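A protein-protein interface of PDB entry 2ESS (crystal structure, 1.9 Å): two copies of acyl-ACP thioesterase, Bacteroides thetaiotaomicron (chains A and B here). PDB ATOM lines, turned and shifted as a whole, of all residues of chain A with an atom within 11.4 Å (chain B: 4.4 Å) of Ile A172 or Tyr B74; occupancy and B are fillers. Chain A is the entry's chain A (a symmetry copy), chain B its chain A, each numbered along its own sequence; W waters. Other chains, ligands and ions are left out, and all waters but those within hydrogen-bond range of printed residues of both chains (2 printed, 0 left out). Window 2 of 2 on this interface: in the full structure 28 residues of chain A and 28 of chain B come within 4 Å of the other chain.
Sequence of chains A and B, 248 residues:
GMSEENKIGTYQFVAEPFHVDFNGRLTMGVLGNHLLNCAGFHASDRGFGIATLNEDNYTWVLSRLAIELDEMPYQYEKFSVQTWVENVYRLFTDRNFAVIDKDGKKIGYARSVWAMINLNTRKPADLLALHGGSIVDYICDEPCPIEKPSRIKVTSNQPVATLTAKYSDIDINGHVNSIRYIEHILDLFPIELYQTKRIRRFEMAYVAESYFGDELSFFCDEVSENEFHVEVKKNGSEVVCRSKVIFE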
ATOM      1  N   ILE A  50     -10.276 -18.142 -18.351  1.00  0.00           N
ATOM      2  CA  ILE A  50      -9.401 -17.028 -18.050  1.00  0.00           C
ATOM      3  C   ILE A  50      -9.778 -15.758 -18.848  1.00  0.00           C
ATOM      4  O   ILE A  50      -9.867 -14.673 -18.287  1.00  0.00           O
ATOM      5  CB  ILE A  50      -7.914 -17.432 -18.279  1.00  0.00           C
ATOM      6  CG1 ILE A  50      -7.501 -18.437 -17.186  1.00  0.00           C
ATOM      7  CG2 ILE A  50      -6.989 -16.158 -18.239  1.00  0.00           C
ATOM      8  CD1 ILE A  50      -6.067 -18.926 -17.219  1.00  0.00           C
ATOM      9  N   ASN A  54     -10.680 -12.270 -17.082  1.00  0.00           N
ATOM     10  CA  ASN A  54      -9.711 -11.169 -17.272  1.00  0.00           C
ATOM     11  C   ASN A  54     -10.391  -9.857 -17.669  1.00  0.00           C
ATOM     12  O   ASN A  54      -9.957  -8.765 -17.270  1.00  0.00           O
ATOM     13  CB  ASN A  54      -8.651 -11.527 -18.345  1.00  0.00           C
ATOM     14  CG  ASN A  54      -7.575 -12.522 -17.898  1.00  0.00           C
ATOM     15  OD1 ASN A  54      -6.760 -12.899 -18.729  1.00  0.00           O
ATOM     16  ND2 ASN A  54      -7.564 -12.958 -16.640  1.00  0.00           N
ATOM     17  N   THR A  59      -8.522 -13.528 -12.425  1.00  0.00           N
ATOM     18  CA  THR A  59      -7.995 -14.669 -13.157  1.00  0.00           C
ATOM     19  C   THR A  59      -8.085 -15.923 -12.289  1.00  0.00           C
ATOM     20  O   THR A  59      -8.408 -15.837 -11.116  1.00  0.00           O
ATOM     21  CB  THR A  59      -6.533 -14.471 -13.674  1.00  0.00           C
ATOM     22  OG1 THR A  59      -6.278 -15.434 -14.685  1.00  0.00           O
ATOM     23  CG2 THR A  59      -5.490 -14.644 -12.525  1.00  0.00           C
ATOM     24  N   TRP A  60      -7.840 -17.071 -12.902  1.00  0.00           N
ATOM     25  CA  TRP A  60      -7.793 -18.354 -12.225  1.00  0.00           C
ATOM     26  C   TRP A  60      -6.356 -18.726 -11.942  1.00  0.00           C
ATOM     27  O   TRP A  60      -5.497 -18.495 -12.794  1.00  0.00           O
ATOM     28  CB  TRP A  60      -8.353 -19.442 -13.138  1.00  0.00           C
ATOM     29  CG  TRP A  60      -9.819 -19.360 -13.403  1.00  0.00           C
ATOM     30  CD1 TRP A  60     -10.417 -19.154 -14.613  1.00  0.00           C
ATOM     31  CD2 TRP A  60     -10.879 -19.576 -12.465  1.00  0.00           C
ATOM     32  NE1 TRP A  60     -11.786 -19.195 -14.480  1.00  0.00           N
ATOM     33  CE2 TRP A  60     -12.097 -19.484 -13.179  1.00  0.00           C
ATOM     34  CE3 TRP A  60     -10.921 -19.881 -11.099  1.00  0.00           C
ATOM     35  CZ2 TRP A  60     -13.336 -19.611 -12.555  1.00  0.00           C
ATOM     36  CZ3 TRP A  60     -12.156 -20.030 -10.483  1.00  0.00           C
ATOM     37  CH2 TRP A  60     -13.344 -19.884 -11.210  1.00  0.00           C
ATOM     38  N   LYS A 166      15.562 -22.637 -16.542  1.00  0.00           N
ATOM     39  CA  LYS A 166      16.131 -22.341 -17.866  1.00  0.00           C
ATOM     40  C   LYS A 166      15.076 -21.887 -18.854  1.00  0.00           C
ATOM     41  O   LYS A 166      13.895 -21.943 -18.561  1.00  0.00           O
ATOM     42  CB  LYS A 166      16.831 -23.585 -18.385  1.00  0.00           C
ATOM     43  CG  LYS A 166      18.116 -23.900 -17.650  1.00  0.00           C
ATOM     44  CD  LYS A 166      18.555 -25.329 -17.895  1.00  0.00           C
ATOM     45  CE  LYS A 166      19.738 -25.710 -16.997  1.00  0.00           C
ATOM     46  NZ  LYS A 166      19.325 -25.974 -15.575  1.00  0.00           N
ATOM     47  N   TYR A 167      15.507 -21.448 -20.032  1.00  0.00           N
ATOM     48  CA  TYR A 167      14.580 -21.052 -21.087  1.00  0.00           C
ATOM     49  C   TYR A 167      13.443 -22.057 -21.318  1.00  0.00           C
ATOM     50  O   TYR A 167      12.287 -21.674 -21.445  1.00  0.00           O
ATOM     51  CB  TYR A 167      15.359 -20.796 -22.376  1.00  0.00           C
ATOM     52  CG  TYR A 167      14.538 -20.561 -23.607  1.00  0.00           C
ATOM     53  CD1 TYR A 167      13.778 -19.407 -23.754  1.00  0.00           C
ATOM     54  CD2 TYR A 167      14.506 -21.507 -24.624  1.00  0.00           C
ATOM     55  CE1 TYR A 167      13.048 -19.185 -24.898  1.00  0.00           C
ATOM     56  CE2 TYR A 167      13.770 -21.309 -25.756  1.00  0.00           C
ATOM     57  CZ  TYR A 167      13.054 -20.147 -25.904  1.00  0.00           C
ATOM     58  OH  TYR A 167      12.306 -19.969 -27.031  1.00  0.00           O
ATOM     59  N   SER A 168      13.746 -23.351 -21.348  1.00  0.00           N
ATOM     60  CA  SER A 168      12.686 -24.342 -21.591  1.00  0.00           C
ATOM     61  C   SER A 168      11.657 -24.471 -20.468  1.00  0.00           C
ATOM     62  O   SER A 168      10.616 -25.065 -20.670  1.00  0.00           O
ATOM     63  CB  SER A 168      13.315 -25.704 -21.807  1.00  0.00           C
ATOM     64  OG  SER A 168      14.155 -25.973 -20.687  1.00  0.00           O
ATOM     65  N   ASP A 169      11.962 -23.966 -19.286  1.00  0.00           N
ATOM     66  CA  ASP A 169      11.045 -24.026 -18.153  1.00  0.00           C
ATOM     67  C   ASP A 169       9.986 -22.941 -18.120  1.00  0.00           C
ATOM     68  O   ASP A 169       8.980 -23.134 -17.457  1.00  0.00           O
ATOM     69  CB  ASP A 169      11.794 -23.971 -16.815  1.00  0.00           C
ATOM     70  CG  ASP A 169      12.703 -25.174 -16.604  1.00  0.00           C
ATOM     71  OD1 ASP A 169      12.212 -26.324 -16.697  1.00  0.00           O
ATOM     72  OD2 ASP A 169      13.918 -24.955 -16.372  1.00  0.00           O
ATOM     73  N   ILE A 170      10.171 -21.851 -18.865  1.00  0.00           N
ATOM     74  CA  ILE A 170       9.423 -20.615 -18.619  1.00  0.00           C
ATOM     75  C   ILE A 170       8.289 -20.442 -19.590  1.00  0.00           C
ATOM     76  O   ILE A 170       8.471 -20.632 -20.790  1.00  0.00           O
ATOM     77  CB  ILE A 170      10.361 -19.401 -18.684  1.00  0.00           C
ATOM     78  CG1 ILE A 170      11.593 -19.629 -17.804  1.00  0.00           C
ATOM     79  CG2 ILE A 170       9.636 -18.079 -18.300  1.00  0.00           C
ATOM     80  CD1 ILE A 170      11.275 -19.783 -16.297  1.00  0.00           C
ATOM     81  N   ASP A 171       7.119 -20.095 -19.052  1.00  0.00           N
ATOM     82  CA  ASP A 171       5.922 -19.794 -19.834  1.00  0.00           C
ATOM     83  C   ASP A 171       5.796 -18.312 -20.194  1.00  0.00           C
ATOM     84  O   ASP A 171       6.708 -17.491 -19.926  1.00  0.00           O
ATOM     85  CB  ASP A 171       4.646 -20.285 -19.095  1.00  0.00           C
ATOM     86  CG  ASP A 171       4.333 -19.492 -17.786  1.00  0.00           C
ATOM     87  OD1 ASP A 171       4.753 -18.330 -17.567  1.00  0.00           O
ATOM     88  OD2 ASP A 171       3.625 -20.079 -16.951  1.00  0.00           O
ATOM     89  N   ILE A 172       4.654 -17.971 -20.790  1.00  0.00           N
ATOM     90  CA  ILE A 172       4.399 -16.619 -21.277  1.00  0.00           C
ATOM     91  C   ILE A 172       4.399 -15.564 -20.173  1.00  0.00           C
ATOM     92  O   ILE A 172       4.659 -14.423 -20.460  1.00  0.00           O
ATOM     93  CB  ILE A 172       3.040 -16.538 -22.032  1.00  0.00           C
ATOM     94  CG1 ILE A 172       2.984 -15.294 -22.929  1.00  0.00           C
ATOM     95  CG2 ILE A 172       1.836 -16.690 -21.030  1.00  0.00           C
ATOM     96  CD1 ILE A 172       1.773 -15.293 -23.930  1.00  0.00           C
ATOM     97  N   ASN A 173       4.105 -15.952 -18.934  1.00  0.00           N
ATOM     98  CA  ASN A 173       4.096 -15.003 -17.821  1.00  0.00           C
ATOM     99  C   ASN A 173       5.449 -14.906 -17.159  1.00  0.00           C
ATOM    100  O   ASN A 173       5.592 -14.217 -16.166  1.00  0.00           O
ATOM    101  CB  ASN A 173       3.055 -15.383 -16.780  1.00  0.00           C
ATOM    102  CG  ASN A 173       1.680 -15.572 -17.385  1.00  0.00           C
ATOM    103  OD1 ASN A 173       1.073 -16.624 -17.240  1.00  0.00           O
ATOM    104  ND2 ASN A 173       1.203 -14.561 -18.097  1.00  0.00           N
ATOM    105  N   GLY A 174       6.448 -15.597 -17.701  1.00  0.00           N
ATOM    106  CA  GLY A 174       7.788 -15.452 -17.174  1.00  0.00           C
ATOM    107  C   GLY A 174       8.035 -16.329 -15.977  1.00  0.00           C
ATOM    108  O   GLY A 174       9.031 -16.157 -15.291  1.00  0.00           O
ATOM    109  N   HIS A 175       7.165 -17.302 -15.724  1.00  0.00           N
ATOM    110  CA  HIS A 175       7.486 -18.187 -14.615  1.00  0.00           C
ATOM    111  C   HIS A 175       7.600 -19.639 -15.058  1.00  0.00           C
ATOM    112  O   HIS A 175       7.196 -20.025 -16.150  1.00  0.00           O
ATOM    113  CB  HIS A 175       6.533 -18.005 -13.424  1.00  0.00           C
ATOM    114  CG  HIS A 175       5.090 -18.168 -13.772  1.00  0.00           C
ATOM    115  ND1 HIS A 175       4.145 -17.200 -13.509  1.00  0.00           N
ATOM    116  CD2 HIS A 175       4.428 -19.194 -14.356  1.00  0.00           C
ATOM    117  CE1 HIS A 175       2.962 -17.621 -13.921  1.00  0.00           C
ATOM    118  NE2 HIS A 175       3.107 -18.824 -14.447  1.00  0.00           N
ATOM    119  N   VAL A 176       8.243 -20.416 -14.199  1.00  0.00           N
ATOM    120  CA  VAL A 176       8.373 -21.823 -14.397  1.00  0.00           C
ATOM    121  C   VAL A 176       6.988 -22.427 -14.422  1.00  0.00           C
ATOM    122  O   VAL A 176       6.184 -22.207 -13.525  1.00  0.00           O
ATOM    123  CB  VAL A 176       9.249 -22.474 -13.310  1.00  0.00           C
ATOM    124  CG1 VAL A 176       9.219 -24.010 -13.466  1.00  0.00           C
ATOM    125  CG2 VAL A 176      10.609 -21.962 -13.434  1.00  0.00           C
ATOM    126  N   ASN A 177       6.692 -23.169 -15.477  1.00  0.00           N
ATOM    127  CA  ASN A 177       5.342 -23.617 -15.675  1.00  0.00           C
ATOM    128  C   ASN A 177       5.004 -24.852 -14.819  1.00  0.00           C
ATOM    129  O   ASN A 177       5.890 -25.570 -14.325  1.00  0.00           O
ATOM    130  CB  ASN A 177       4.985 -23.661 -17.189  1.00  0.00           C
ATOM    131  CG  ASN A 177       5.341 -24.953 -17.874  1.00  0.00           C
ATOM    132  OD1 ASN A 177       5.150 -26.008 -17.326  1.00  0.00           O
ATOM    133  ND2 ASN A 177       5.782 -24.867 -19.142  1.00  0.00           N
ATOM    134  N   SER A 178       3.708 -25.018 -14.586  1.00  0.00           N
ATOM    135  CA  SER A 178       3.159 -26.079 -13.756  1.00  0.00           C
ATOM    136  C   SER A 178       3.672 -27.477 -14.074  1.00  0.00           C
ATOM    137  O   SER A 178       3.946 -28.288 -13.165  1.00  0.00           O
ATOM    138  CB  SER A 178       1.643 -26.110 -13.958  1.00  0.00           C
ATOM    139  OG  SER A 178       1.077 -24.885 -13.610  1.00  0.00           O
ATOM    140  N   ILE A 179       3.794 -27.752 -15.375  1.00  0.00           N
ATOM    141  CA  ILE A 179       4.190 -29.058 -15.876  1.00  0.00           C
ATOM    142  C   ILE A 179       5.681 -29.301 -15.732  1.00  0.00           C
ATOM    143  O   ILE A 179       6.110 -30.425 -15.505  1.00  0.00           O
ATOM    144  CB  ILE A 179       3.770 -29.211 -17.365  1.00  0.00           C
ATOM    145  CG1 ILE A 179       2.267 -29.031 -17.493  1.00  0.00           C
ATOM    146  CG2 ILE A 179       4.131 -30.566 -17.908  1.00  0.00           C
ATOM    147  CD1 ILE A 179       1.481 -29.827 -16.495  1.00  0.00           C
ATOM    148  N   ARG A 180       6.482 -28.255 -15.880  1.00  0.00           N
ATOM    149  CA  ARG A 180       7.907 -28.389 -15.744  1.00  0.00           C
ATOM    150  C   ARG A 180       8.278 -28.762 -14.324  1.00  0.00           C
ATOM    151  O   ARG A 180       9.198 -29.537 -14.133  1.00  0.00           O
ATOM    152  CB  ARG A 180       8.616 -27.103 -16.162  1.00  0.00           C
ATOM    153  CG  ARG A 180       8.526 -26.864 -17.667  1.00  0.00           C
ATOM    154  CD  ARG A 180       9.466 -27.782 -18.394  1.00  0.00           C
ATOM    155  NE  ARG A 180       9.135 -27.878 -19.806  1.00  0.00           N
ATOM    156  CZ  ARG A 180       9.877 -28.551 -20.690  1.00  0.00           C
ATOM    157  NH1 ARG A 180      10.997 -29.161 -20.306  1.00  0.00           N
ATOM    158  NH2 ARG A 180       9.511 -28.600 -21.965  1.00  0.00           N
ATOM    159  N   GLU A 209       5.864 -18.640  -7.199  1.00  0.00           N
ATOM    160  CA  GLU A 209       6.407 -18.638  -8.547  1.00  0.00           C
ATOM    161  C   GLU A 209       7.911 -18.623  -8.524  1.00  0.00           C
ATOM    162  O   GLU A 209       8.510 -18.085  -7.610  1.00  0.00           O
ATOM    163  CB  GLU A 209       5.905 -17.421  -9.346  1.00  0.00           C
ATOM    164  CG  GLU A 209       4.419 -17.328  -9.480  1.00  0.00           C
ATOM    165  CD  GLU A 209       3.771 -18.423 -10.367  1.00  0.00           C
ATOM    166  OE1 GLU A 209       4.454 -19.389 -10.784  1.00  0.00           O
ATOM    167  OE2 GLU A 209       2.549 -18.314 -10.651  1.00  0.00           O
ATOM    168  N   SER A 210       8.496 -19.234  -9.555  1.00  0.00           N
ATOM    169  CA  SER A 210       9.931 -19.195  -9.835  1.00  0.00           C
ATOM    170  C   SER A 210      10.131 -18.576 -11.207  1.00  0.00           C
ATOM    171  O   SER A 210       9.278 -18.715 -12.087  1.00  0.00           O
ATOM    172  CB  SER A 210      10.520 -20.607  -9.879  1.00  0.00           C
ATOM    173  OG  SER A 210      10.397 -21.203  -8.615  1.00  0.00           O
ATOM    174  N   TYR A 211      11.280 -17.940 -11.378  1.00  0.00           N
ATOM    175  CA  TYR A 211      11.616 -17.204 -12.584  1.00  0.00           C
ATOM    176  C   TYR A 211      12.902 -17.758 -13.209  1.00  0.00           C
ATOM    177  O   TYR A 211      13.655 -18.543 -12.587  1.00  0.00           O
ATOM    178  CB  TYR A 211      11.820 -15.744 -12.225  1.00  0.00           C
ATOM    179  CG  TYR A 211      10.634 -15.192 -11.476  1.00  0.00           C
ATOM    180  CD1 TYR A 211       9.474 -14.862 -12.137  1.00  0.00           C
ATOM    181  CD2 TYR A 211      10.664 -15.058 -10.095  1.00  0.00           C
ATOM    182  CE1 TYR A 211       8.356 -14.374 -11.437  1.00  0.00           C
ATOM    183  CE2 TYR A 211       9.557 -14.576  -9.386  1.00  0.00           C
ATOM    184  CZ  TYR A 211       8.413 -14.242 -10.064  1.00  0.00           C
ATOM    185  OH  TYR A 211       7.336 -13.764  -9.369  1.00  0.00           O
ATOM    186  N   PHE A 212      13.166 -17.311 -14.423  1.00  0.00           N
ATOM    187  CA  PHE A 212      14.377 -17.704 -15.131  1.00  0.00           C
ATOM    188  C   PHE A 212      15.607 -17.361 -14.311  1.00  0.00           C
ATOM    189  O   PHE A 212      15.712 -16.256 -13.793  1.00  0.00           O
ATOM    190  CB  PHE A 212      14.479 -16.984 -16.477  1.00  0.00           C
ATOM    191  CG  PHE A 212      15.805 -17.190 -17.154  1.00  0.00           C
ATOM    192  CD1 PHE A 212      16.896 -16.351 -16.863  1.00  0.00           C
ATOM    193  CD2 PHE A 212      15.965 -18.220 -18.050  1.00  0.00           C
ATOM    194  CE1 PHE A 212      18.149 -16.554 -17.462  1.00  0.00           C
ATOM    195  CE2 PHE A 212      17.196 -18.441 -18.661  1.00  0.00           C
ATOM    196  CZ  PHE A 212      18.296 -17.602 -18.374  1.00  0.00           C
ATOM    197  N   ALA B  15      -1.569 -23.788 -30.752  1.00  0.00           N
ATOM    198  CA  ALA B  15      -0.431 -23.553 -29.847  1.00  0.00           C
ATOM    199  C   ALA B  15      -0.878 -23.468 -28.352  1.00  0.00           C
ATOM    200  O   ALA B  15      -1.440 -22.476 -27.905  1.00  0.00           O
ATOM    201  CB  ALA B  15       0.317 -22.288 -30.257  1.00  0.00           C
ATOM    202  N   ASP B  21       7.026 -20.235 -25.362  1.00  0.00           N
ATOM    203  CA  ASP B  21       8.071 -19.617 -24.549  1.00  0.00           C
ATOM    204  C   ASP B  21       7.611 -18.329 -23.890  1.00  0.00           C
ATOM    205  O   ASP B  21       6.420 -17.984 -23.946  1.00  0.00           O
ATOM    206  CB  ASP B  21       9.357 -19.400 -25.368  1.00  0.00           C
ATOM    207  CG  ASP B  21       9.187 -18.400 -26.557  1.00  0.00           C
ATOM    208  OD1 ASP B  21       8.246 -17.568 -26.565  1.00  0.00           O
ATOM    209  OD2 ASP B  21      10.034 -18.485 -27.487  1.00  0.00           O
ATOM    210  N   PHE B  22       8.551 -17.628 -23.249  1.00  0.00           N
ATOM    211  CA  PHE B  22       8.208 -16.432 -22.513  1.00  0.00           C
ATOM    212  C   PHE B  22       7.712 -15.284 -23.392  1.00  0.00           C
ATOM    213  O   PHE B  22       7.100 -14.357 -22.864  1.00  0.00           O
ATOM    214  CB  PHE B  22       9.339 -15.959 -21.600  1.00  0.00           C
ATOM    215  CG  PHE B  22      10.513 -15.404 -22.330  1.00  0.00           C
ATOM    216  CD1 PHE B  22      10.576 -14.051 -22.654  1.00  0.00           C
ATOM    217  CD2 PHE B  22      11.555 -16.234 -22.723  1.00  0.00           C
ATOM    218  CE1 PHE B  22      11.664 -13.529 -23.330  1.00  0.00           C
ATOM    219  CE2 PHE B  22      12.663 -15.707 -23.387  1.00  0.00           C
ATOM    220  CZ  PHE B  22      12.716 -14.361 -23.700  1.00  0.00           C
ATOM    221  N   ASN B  23       7.941 -15.367 -24.704  1.00  0.00           N
ATOM    222  CA  ASN B  23       7.326 -14.398 -25.655  1.00  0.00           C
ATOM    223  C   ASN B  23       5.988 -14.905 -26.241  1.00  0.00           C
ATOM    224  O   ASN B  23       5.405 -14.257 -27.110  1.00  0.00           O
ATOM    225  CB  ASN B  23       8.256 -14.067 -26.809  1.00  0.00           C
ATOM    226  CG  ASN B  23       9.526 -13.321 -26.383  1.00  0.00           C
ATOM    227  OD1 ASN B  23       9.501 -12.384 -25.592  1.00  0.00           O
ATOM    228  ND2 ASN B  23      10.659 -13.774 -26.933  1.00  0.00           N
ATOM    229  N   GLY B  24       5.492 -16.026 -25.733  1.00  0.00           N
ATOM    230  CA  GLY B  24       4.210 -16.607 -26.178  1.00  0.00           C
ATOM    231  C   GLY B  24       4.258 -17.336 -27.511  1.00  0.00           C
ATOM    232  O   GLY B  24       3.236 -17.585 -28.102  1.00  0.00           O
ATOM    233  N   ARG B  25       5.450 -17.654 -28.000  1.00  0.00           N
ATOM    234  CA  ARG B  25       5.623 -18.306 -29.303  1.00  0.00           C
ATOM    235  C   ARG B  25       5.972 -19.742 -29.093  1.00  0.00           C
ATOM    236  O   ARG B  25       6.708 -20.066 -28.169  1.00  0.00           O
ATOM    237  CB  ARG B  25       6.796 -17.678 -30.065  1.00  0.00           C
ATOM    238  CG  ARG B  25       6.659 -16.200 -30.316  1.00  0.00           C
ATOM    239  CD  ARG B  25       5.723 -15.983 -31.445  1.00  0.00           C
ATOM    240  NE  ARG B  25       5.252 -14.612 -31.511  1.00  0.00           N
ATOM    241  CZ  ARG B  25       4.462 -14.145 -32.466  1.00  0.00           C
ATOM    242  NH1 ARG B  25       4.096 -14.927 -33.463  1.00  0.00           N
ATOM    243  NH2 ARG B  25       4.049 -12.872 -32.433  1.00  0.00           N
ATOM    244  N   MET B  72       6.791 -17.800 -35.768  1.00  0.00           N
ATOM    245  CA  MET B  72       6.379 -18.979 -35.024  1.00  0.00           C
ATOM    246  C   MET B  72       4.920 -18.723 -34.602  1.00  0.00           C
ATOM    247  O   MET B  72       4.568 -17.609 -34.253  1.00  0.00           O
ATOM    248  CB  MET B  72       7.294 -19.023 -33.800  1.00  0.00           C
ATOM    249  CG  MET B  72       7.505 -20.286 -33.119  1.00  0.00           C
ATOM    250  SD  MET B  72       7.895 -21.858 -34.220  1.00  0.00           S
ATOM    251  CE  MET B  72       9.446 -22.553 -33.220  1.00  0.00           C
ATOM    252  N   PRO B  73       4.073 -19.748 -34.574  1.00  0.00           N
ATOM    253  CA  PRO B  73       2.716 -19.495 -34.053  1.00  0.00           C
ATOM    254  C   PRO B  73       2.674 -18.936 -32.620  1.00  0.00           C
ATOM    255  O   PRO B  73       3.521 -19.292 -31.798  1.00  0.00           O
ATOM    256  CB  PRO B  73       2.094 -20.886 -34.042  1.00  0.00           C
ATOM    257  CG  PRO B  73       2.852 -21.667 -34.964  1.00  0.00           C
ATOM    258  CD  PRO B  73       4.255 -21.132 -35.002  1.00  0.00           C
ATOM    259  N   TYR B  74       1.672 -18.119 -32.334  1.00  0.00           N
ATOM    260  CA  TYR B  74       1.457 -17.544 -31.008  1.00  0.00           C
ATOM    261  C   TYR B  74       0.479 -18.361 -30.154  1.00  0.00           C
ATOM    262  O   TYR B  74      -0.389 -19.073 -30.667  1.00  0.00           O
ATOM    263  CB  TYR B  74       0.965 -16.102 -31.154  1.00  0.00           C
ATOM    264  CG  TYR B  74       0.894 -15.312 -29.870  1.00  0.00           C
ATOM    265  CD1 TYR B  74       2.010 -14.658 -29.377  1.00  0.00           C
ATOM    266  CD2 TYR B  74      -0.299 -15.202 -29.161  1.00  0.00           C
ATOM    267  CE1 TYR B  74       1.951 -13.905 -28.204  1.00  0.00           C
ATOM    268  CE2 TYR B  74      -0.373 -14.462 -27.969  1.00  0.00           C
ATOM    269  CZ  TYR B  74       0.765 -13.818 -27.496  1.00  0.00           C
ATOM    270  OH  TYR B  74       0.727 -13.076 -26.347  1.00  0.00           O
ATOM    271  N   GLN B  75       0.618 -18.239 -28.835  1.00  0.00           N
ATOM    272  CA  GLN B  75      -0.221 -18.938 -27.887  1.00  0.00           C
ATOM    273  C   GLN B  75      -1.688 -18.856 -28.286  1.00  0.00           C
ATOM    274  O   GLN B  75      -2.185 -17.785 -28.591  1.00  0.00           O
ATOM    275  CB  GLN B  75      -0.035 -18.348 -26.483  1.00  0.00           C
ATOM    276  CG  GLN B  75      -0.713 -19.149 -25.420  1.00  0.00           C
ATOM    277  CD  GLN B  75      -0.484 -18.588 -24.027  1.00  0.00           C
ATOM    278  OE1 GLN B  75       0.352 -19.078 -23.289  1.00  0.00           O
ATOM    279  NE2 GLN B  75      -1.200 -17.538 -23.691  1.00  0.00           N
ATOM    280  N   TYR B  76      -2.345 -20.015 -28.299  1.00  0.00           N
ATOM    281  CA  TYR B  76      -3.756 -20.180 -28.678  1.00  0.00           C
ATOM    282  C   TYR B  76      -4.144 -19.982 -30.156  1.00  0.00           C
ATOM    283  O   TYR B  76      -5.309 -20.125 -30.492  1.00  0.00           O
ATOM    284  CB  TYR B  76      -4.672 -19.336 -27.806  1.00  0.00           C
ATOM    285  CG  TYR B  76      -4.715 -19.773 -26.379  1.00  0.00           C
ATOM    286  CD1 TYR B  76      -5.039 -21.090 -26.036  1.00  0.00           C
ATOM    287  CD2 TYR B  76      -4.433 -18.882 -25.378  1.00  0.00           C
ATOM    288  CE1 TYR B  76      -5.087 -21.481 -24.714  1.00  0.00           C
ATOM    289  CE2 TYR B  76      -4.470 -19.251 -24.066  1.00  0.00           C
ATOM    290  CZ  TYR B  76      -4.791 -20.534 -23.733  1.00  0.00           C
ATOM    291  OH  TYR B  76      -4.820 -20.841 -22.403  1.00  0.00           O
ATOM    292  N   GLU B  77      -3.179 -19.721 -31.031  1.00  0.00           N
ATOM    293  CA  GLU B  77      -3.465 -19.630 -32.450  1.00  0.00           C
ATOM    294  C   GLU B  77      -3.497 -21.011 -33.064  1.00  0.00           C
ATOM    295  O   GLU B  77      -2.743 -21.898 -32.675  1.00  0.00           O
ATOM    296  CB  GLU B  77      -2.401 -18.842 -33.184  1.00  0.00           C
ATOM    297  CG  GLU B  77      -2.291 -17.416 -32.822  1.00  0.00           C
ATOM    298  CD  GLU B  77      -1.325 -16.656 -33.749  1.00  0.00           C
ATOM    299  OE1 GLU B  77      -0.369 -17.272 -34.369  1.00  0.00           O
ATOM    300  OE2 GLU B  77      -1.540 -15.431 -33.844  1.00  0.00           O
HETATM  301  O   HOH W   1       2.273 -19.863 -21.610  1.00  0.00           O
HETATM  302  O   HOH W   2      10.619 -19.613 -22.389  1.00  0.00           O
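The side-chain carboxylate of Asp B21 lies within hydrogen-bond range of the side-chain hydroxyl of Tyr A167 (2.8 Å). The backbone carbonyl oxygen (O) of Phe B22 sits close to the backbone carbonyl oxygen (O) of Ile A172 (3.4 Å).
N of Gly A174 is in hydrogen-bond range of OD1 of Asp A171. The backbone NH (N) of Asn B23 is in hydrogen-bond range of the side-chain carboxylate (OD1) of Asp B21. N of Tyr B74 is in hydrogen-bond range of OE1 of Glu B77 (3.0 Å). O of Gly B24 sits at hydrogen-bond distance from N of Gln B75, at 2.8 Å. The side-chain carboxylate of Asp B21 is in hydrogen-bond range of the backbone NH of Gly B24 (3.3 Å). OD1 of Asp A171 is in hydrogen-bond range of N of Asn A173 (2.8 Å).
Tyr A167 touches Phe B22. Asp B21 touches Ile A170 (CA to O, 3.9 Å). Ile A170 touches Phe B22. Asp A171 touches Asp B21. Asp A171 touches Phe B22 (O to CA, 3.2 Å). O of Asp B21 touches CA of Ile A172, at 3.6 Å. Ile A172 touches Gly B24. OH of Tyr B74 touches CD1 of Ile A172, at 3.4 Å. Ile A172 touches Gln B75 (CG2 to OE1, 3.6 Å).
Of the printed residues of chain B, Ile A170 touches Asp B21 and Phe B22. Of the printed residues of chain B, Asp A171 touches Asp B21 and Phe B22. Ile A172 touches just these residues of chain B: Asp B21 (3.6 Å), Phe B22 (3.4 Å), Gly B24 (3.6 Å), Tyr B74 (3.4 Å) and Gln B75 (3.6 Å). Ser A178 touches none of the printed residues of chain B. Tyr A211 touches none of the printed residues of chain B. No residue of chain A comes within 4 Å of Ala B15. Of the printed residues of chain A, Phe B22 touches Tyr A167 (3.8 Å), Ile A170 (3.9 Å), Asp A171 (3.2 Å) and Ile A172 (3.4 Å). Of the printed residues of chain A, Gly B24 touches Ile A172. No residue of chain A comes within 4 Å of Arg B25. No residue of chain A comes within 4 Å of Pro B73. Tyr B74 touches just one residue of chain A: Ile A172 (3.4 Å). The nearest printed residue of chain B that does not touch Ile A172 is Asn B23 (4.5 Å).
Of the 23 printed residues of chain A, 4 touch a printed residue of chain B. Printed residues of chain A that touch a printed residue of chain B: Tyr A167, Ile A170, Asp A171 and Ile A172. Of the 12 printed residues of chain B, 5 touch a printed residue of chain A. Hydrophobic or aromatic side chains of chain B that line the printed part of chain A: Phe B22 and Tyr B74. Among the printed residues, 11 pairs touch across the chains.
No position is printed for both chains.
Water W1 lies within hydrogen-bond range of the side-chain amide oxygen (OE1) of Gln B75 (2.7 Å) and the backbone NH (N) of Ile A172 (3.1 Å). Water W2 lies within hydrogen-bond range of the backbone carbonyl oxygen of Tyr A167 (2.8 Å), the backbone carbonyl oxygen of Ile A170 (2.9 Å) and the backbone NH of Phe B22 (3.0 Å).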
